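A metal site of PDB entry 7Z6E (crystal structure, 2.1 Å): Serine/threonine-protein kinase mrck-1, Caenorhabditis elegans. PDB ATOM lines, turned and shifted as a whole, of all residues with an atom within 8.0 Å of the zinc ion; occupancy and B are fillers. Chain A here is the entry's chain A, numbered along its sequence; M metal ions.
Of the 21 residues printed, 4 come within 4 Å of the zinc ion.
Along chain A the residues within 4 Å of the zinc ion span positions 19 to 47.
The side-chain sulfur (SG) of Cys 22 sits close to the side-chain hydroxyl (OG) of Ser 24 (3.4 Å).
The backbone NH of Cys 19 is in hydrogen-bond range of the backbone carbonyl oxygen of Ser 24, at 2.6 Å.
SG of Cys 19 lies close to N of His 21, at 3.3 Å.
NE2 of His 44 is in hydrogen-bond range of O of Ile 25, 3.4 Å away.
The zinc ion is bound by a ring nitrogen (ND1) of His 44, 2.1 Å away.
The zinc ion is bound by SG of Cys 47 (2.3 Å).
The side-chain sulfur (SG) of Cys 22 binds the zinc ion (2.4 Å).
SG of Cys 19 is bound to the zinc ion (2.4 Å).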
ATOM      1  N   LYS A  18      -4.180  -1.422   7.169  1.00  0.00           N
ATOM      2  CA  LYS A  18      -4.710  -1.554   8.516  1.00  0.00           C
ATOM      3  C   LYS A  18      -3.782  -0.954   9.568  1.00  0.00           C
ATOM      4  O   LYS A  18      -2.549  -1.132   9.511  1.00  0.00           O
ATOM      5  CB  LYS A  18      -4.967  -3.031   8.824  1.00  0.00           C
ATOM      6  CG  LYS A  18      -5.728  -3.732   7.721  1.00  0.00           C
ATOM      7  CD  LYS A  18      -6.387  -4.991   8.223  1.00  0.00           C
ATOM      8  CE  LYS A  18      -5.389  -6.132   8.343  1.00  0.00           C
ATOM      9  NZ  LYS A  18      -5.410  -7.020   7.149  1.00  0.00           N
ATOM     10  N   CYS A  19      -4.367  -0.241  10.522  1.00  0.00           N
ATOM     11  CA  CYS A  19      -3.612   0.186  11.699  1.00  0.00           C
ATOM     12  C   CYS A  19      -3.055  -1.045  12.397  1.00  0.00           C
ATOM     13  O   CYS A  19      -3.787  -1.992  12.704  1.00  0.00           O
ATOM     14  CB  CYS A  19      -4.499   0.974  12.652  1.00  0.00           C
ATOM     15  SG  CYS A  19      -3.642   1.503  14.140  1.00  0.00           S
ATOM     16  N   GLY A  20      -1.755  -1.031  12.676  1.00  0.00           N
ATOM     17  CA  GLY A  20      -1.192  -2.166  13.379  1.00  0.00           C
ATOM     18  C   GLY A  20      -1.697  -2.309  14.797  1.00  0.00           C
ATOM     19  O   GLY A  20      -1.579  -3.382  15.385  1.00  0.00           O
ATOM     20  N   HIS A  21      -2.262  -1.251  15.359  1.00  0.00           N
ATOM     21  CA  HIS A  21      -2.745  -1.381  16.727  1.00  0.00           C
ATOM     22  C   HIS A  21      -4.230  -1.725  16.796  1.00  0.00           C
ATOM     23  O   HIS A  21      -4.612  -2.553  17.622  1.00  0.00           O
ATOM     24  CB  HIS A  21      -2.465  -0.095  17.499  1.00  0.00           C
ATOM     25  CG  HIS A  21      -2.914  -0.138  18.921  1.00  0.00           C
ATOM     26  ND1 HIS A  21      -4.081   0.457  19.350  1.00  0.00           N
ATOM     27  CD2 HIS A  21      -2.355  -0.703  20.022  1.00  0.00           C
ATOM     28  CE1 HIS A  21      -4.223   0.265  20.643  1.00  0.00           C
ATOM     29  NE2 HIS A  21      -3.188  -0.436  21.081  1.00  0.00           N
ATOM     30  N   CYS A  22      -5.085  -1.132  15.970  1.00  0.00           N
ATOM     31  CA  CYS A  22      -6.513  -1.372  16.084  1.00  0.00           C
ATOM     32  C   CYS A  22      -7.100  -2.094  14.877  1.00  0.00           C
ATOM     33  O   CYS A  22      -8.255  -2.517  14.942  1.00  0.00           O
ATOM     34  CB  CYS A  22      -7.284  -0.061  16.315  1.00  0.00           C
ATOM     35  SG  CYS A  22      -7.401   0.995  14.856  1.00  0.00           S
ATOM     36  N   THR A  23      -6.321  -2.252  13.800  1.00  0.00           N
ATOM     37  CA  THR A  23      -6.646  -2.943  12.541  1.00  0.00           C
ATOM     38  C   THR A  23      -7.579  -2.162  11.628  1.00  0.00           C
ATOM     39  O   THR A  23      -7.829  -2.633  10.518  1.00  0.00           O
ATOM     40  CB  THR A  23      -7.239  -4.346  12.730  1.00  0.00           C
ATOM     41  OG1 THR A  23      -8.629  -4.223  13.046  1.00  0.00           O
ATOM     42  CG2 THR A  23      -6.482  -5.153  13.813  1.00  0.00           C
ATOM     43  N   SER A  24      -8.078  -1.000  12.034  1.00  0.00           N
ATOM     44  CA  SER A  24      -8.874  -0.182  11.135  1.00  0.00           C
ATOM     45  C   SER A  24      -8.006   0.382  10.005  1.00  0.00           C
ATOM     46  O   SER A  24      -6.823   0.681  10.190  1.00  0.00           O
ATOM     47  CB  SER A  24      -9.563   0.972  11.877  1.00  0.00           C
ATOM     48  OG  SER A  24     -10.225   0.516  13.030  1.00  0.00           O
ATOM     49  N   ILE A  25      -8.614   0.494   8.824  1.00  0.00           N
ATOM     50  CA  ILE A  25      -7.933   1.125   7.694  1.00  0.00           C
ATOM     51  C   ILE A  25      -7.551   2.549   8.070  1.00  0.00           C
ATOM     52  O   ILE A  25      -8.318   3.264   8.723  1.00  0.00           O
ATOM     53  CB  ILE A  25      -8.836   1.102   6.450  1.00  0.00           C
ATOM     54  CG1 ILE A  25      -9.198  -0.346   6.076  1.00  0.00           C
ATOM     55  CG2 ILE A  25      -8.160   1.843   5.292  1.00  0.00           C
ATOM     56  CD1 ILE A  25      -7.974  -1.237   5.735  1.00  0.00           C
ATOM     57  N   LEU A  26      -6.338   2.950   7.683  1.00  0.00           N
ATOM     58  CA  LEU A  26      -5.854   4.323   7.852  1.00  0.00           C
ATOM     59  C   LEU A  26      -6.409   5.160   6.698  1.00  0.00           C
ATOM     60  O   LEU A  26      -5.762   5.381   5.673  1.00  0.00           O
ATOM     61  CB  LEU A  26      -4.327   4.358   7.877  1.00  0.00           C
ATOM     62  CG  LEU A  26      -3.637   3.424   8.881  1.00  0.00           C
ATOM     63  CD1 LEU A  26      -2.174   3.102   8.456  1.00  0.00           C
ATOM     64  CD2 LEU A  26      -3.710   4.007  10.302  1.00  0.00           C
ATOM     65  N   TYR A  41       6.174  -0.485  11.337  1.00  0.00           N
ATOM     66  CA  TYR A  41       4.856  -0.417  11.948  1.00  0.00           C
ATOM     67  C   TYR A  41       4.111   0.821  11.455  1.00  0.00           C
ATOM     68  O   TYR A  41       4.689   1.925  11.401  1.00  0.00           O
ATOM     69  CB  TYR A  41       5.019  -0.398  13.471  1.00  0.00           C
ATOM     70  CG  TYR A  41       3.798  -0.670  14.310  1.00  0.00           C
ATOM     71  CD1 TYR A  41       3.440  -1.967  14.655  1.00  0.00           C
ATOM     72  CD2 TYR A  41       3.032   0.371  14.813  1.00  0.00           C
ATOM     73  CE1 TYR A  41       2.316  -2.216  15.447  1.00  0.00           C
ATOM     74  CE2 TYR A  41       1.909   0.136  15.602  1.00  0.00           C
ATOM     75  CZ  TYR A  41       1.560  -1.157  15.911  1.00  0.00           C
ATOM     76  OH  TYR A  41       0.467  -1.394  16.705  1.00  0.00           O
ATOM     77  N   ALA A  42       2.834   0.661  11.084  1.00  0.00           N
ATOM     78  CA  ALA A  42       1.982   1.780  10.687  1.00  0.00           C
ATOM     79  C   ALA A  42       0.763   1.840  11.586  1.00  0.00           C
ATOM     80  O   ALA A  42       0.181   0.798  11.908  1.00  0.00           O
ATOM     81  CB  ALA A  42       1.542   1.653   9.229  1.00  0.00           C
ATOM     82  N   CYS A  43       0.351   3.051  12.002  1.00  0.00           N
ATOM     83  CA  CYS A  43      -0.771   3.157  12.932  1.00  0.00           C
ATOM     84  C   CYS A  43      -1.351   4.567  12.939  1.00  0.00           C
ATOM     85  O   CYS A  43      -0.698   5.546  12.566  1.00  0.00           O
ATOM     86  CB  CYS A  43      -0.350   2.769  14.362  1.00  0.00           C
ATOM     87  SG  CYS A  43       0.895   3.876  15.078  1.00  0.00           S
ATOM     88  N   HIS A  44      -2.615   4.652  13.387  1.00  0.00           N
ATOM     89  CA  HIS A  44      -3.259   5.939  13.620  1.00  0.00           C
ATOM     90  C   HIS A  44      -2.444   6.740  14.621  1.00  0.00           C
ATOM     91  O   HIS A  44      -1.876   6.180  15.561  1.00  0.00           O
ATOM     92  CB  HIS A  44      -4.688   5.766  14.180  1.00  0.00           C
ATOM     93  CG  HIS A  44      -5.655   5.142  13.215  1.00  0.00           C
ATOM     94  ND1 HIS A  44      -6.028   3.806  13.288  1.00  0.00           N
ATOM     95  CD2 HIS A  44      -6.330   5.653  12.152  1.00  0.00           C
ATOM     96  CE1 HIS A  44      -6.860   3.529  12.309  1.00  0.00           C
ATOM     97  NE2 HIS A  44      -7.052   4.633  11.601  1.00  0.00           N
ATOM     98  N   VAL A  45      -2.382   8.049  14.398  1.00  0.00           N
ATOM     99  CA  VAL A  45      -1.762   8.971  15.354  1.00  0.00           C
ATOM    100  C   VAL A  45      -2.365   8.783  16.741  1.00  0.00           C
ATOM    101  O   VAL A  45      -1.643   8.723  17.748  1.00  0.00           O
ATOM    102  CB  VAL A  45      -1.908  10.434  14.858  1.00  0.00           C
ATOM    103  CG1 VAL A  45      -1.344  11.431  15.859  1.00  0.00           C
ATOM    104  CG2 VAL A  45      -1.224  10.613  13.489  1.00  0.00           C
ATOM    105  N   SER A  46      -3.682   8.658  16.823  1.00  0.00           N
ATOM    106  CA  SER A  46      -4.299   8.476  18.126  1.00  0.00           C
ATOM    107  C   SER A  46      -4.020   7.092  18.701  1.00  0.00           C
ATOM    108  O   SER A  46      -4.146   6.906  19.916  1.00  0.00           O
ATOM    109  CB  SER A  46      -5.812   8.706  18.028  1.00  0.00           C
ATOM    110  OG  SER A  46      -6.396   7.686  17.227  1.00  0.00           O
ATOM    111  N   CYS A  47      -3.680   6.109  17.870  1.00  0.00           N
ATOM    112  CA  CYS A  47      -3.364   4.774  18.371  1.00  0.00           C
ATOM    113  C   CYS A  47      -1.929   4.659  18.856  1.00  0.00           C
ATOM    114  O   CYS A  47      -1.646   3.829  19.726  1.00  0.00           O
ATOM    115  CB  CYS A  47      -3.619   3.727  17.278  1.00  0.00           C
ATOM    116  SG  CYS A  47      -5.356   3.388  17.007  1.00  0.00           S
ATOM    117  N   ALA A  48      -1.024   5.480  18.305  1.00  0.00           N
ATOM    118  CA  ALA A  48       0.384   5.423  18.675  1.00  0.00           C
ATOM    119  C   ALA A  48       0.596   5.521  20.177  1.00  0.00           C
ATOM    120  O   ALA A  48       1.477   4.860  20.742  1.00  0.00           O
ATOM    121  CB  ALA A  48       1.153   6.532  17.958  1.00  0.00           C
ATOM    122  N   ARG A  50      -0.813   4.261  22.584  1.00  0.00           N
ATOM    123  CA  ARG A  50      -1.019   3.021  23.304  1.00  0.00           C
ATOM    124  C   ARG A  50      -0.258   1.849  22.700  1.00  0.00           C
ATOM    125  O   ARG A  50      -0.379   0.725  23.203  1.00  0.00           O
ATOM    126  CB  ARG A  50      -2.514   2.695  23.381  1.00  0.00           C
ATOM    127  CG  ARG A  50      -3.266   3.463  24.460  1.00  0.00           C
ATOM    128  CD  ARG A  50      -4.771   3.402  24.246  1.00  0.00           C
ATOM    129  NE  ARG A  50      -5.218   4.341  23.223  1.00  0.00           N
ATOM    130  CZ  ARG A  50      -5.917   4.008  22.136  1.00  0.00           C
ATOM    131  NH1 ARG A  50      -6.273   2.749  21.911  1.00  0.00           N
ATOM    132  NH2 ARG A  50      -6.264   4.955  21.270  1.00  0.00           N
ATOM    133  N   VAL A  51       0.536   2.071  21.645  1.00  0.00           N
ATOM    134  CA  VAL A  51       1.392   1.026  21.125  1.00  0.00           C
ATOM    135  C   VAL A  51       2.560   0.797  22.075  1.00  0.00           C
ATOM    136  O   VAL A  51       3.068   1.738  22.702  1.00  0.00           O
ATOM    137  CB  VAL A  51       1.913   1.392  19.718  1.00  0.00           C
ATOM    138  CG1 VAL A  51       2.600   0.194  19.084  1.00  0.00           C
ATOM    139  CG2 VAL A  51       0.774   1.860  18.846  1.00  0.00           C
ATOM    140  N   ARG A  71     -17.092   0.076  20.864  1.00  0.00           N
ATOM    141  CA  ARG A  71     -16.283   1.136  20.247  1.00  0.00           C
ATOM    142  C   ARG A  71     -16.411   1.041  18.727  1.00  0.00           C
ATOM    143  O   ARG A  71     -16.217   2.038  18.031  1.00  0.00           O
ATOM    144  CB  ARG A  71     -14.804   1.092  20.683  1.00  0.00           C
ATOM    145  CG  ARG A  71     -14.198   2.441  21.034  1.00  0.00           C
ATOM    146  CD  ARG A  71     -12.775   2.305  21.548  1.00  0.00           C
ATOM    147  NE  ARG A  71     -11.895   1.630  20.598  1.00  0.00           N
ATOM    148  CZ  ARG A  71     -11.149   2.245  19.691  1.00  0.00           C
ATOM    149  NH1 ARG A  71     -11.148   3.566  19.571  1.00  0.00           N
ATOM    150  NH2 ARG A  71     -10.374   1.521  18.880  1.00  0.00           N
ATOM    151  N   VAL A  73     -14.744  -0.883  16.122  1.00  0.00           N
ATOM    152  CA  VAL A  73     -13.477  -0.648  15.452  1.00  0.00           C
ATOM    153  C   VAL A  73     -12.894  -1.969  14.977  1.00  0.00           C
ATOM    154  O   VAL A  73     -12.897  -2.959  15.726  1.00  0.00           O
ATOM    155  CB  VAL A  73     -12.498   0.114  16.388  1.00  0.00           C
ATOM    156  CG1 VAL A  73     -11.042  -0.180  16.031  1.00  0.00           C
ATOM    157  CG2 VAL A  73     -12.776   1.603  16.366  1.00  0.00           C
HETATM  158 ZN    ZN M   1      -5.611   2.522  14.937  1.00  0.00          ZN
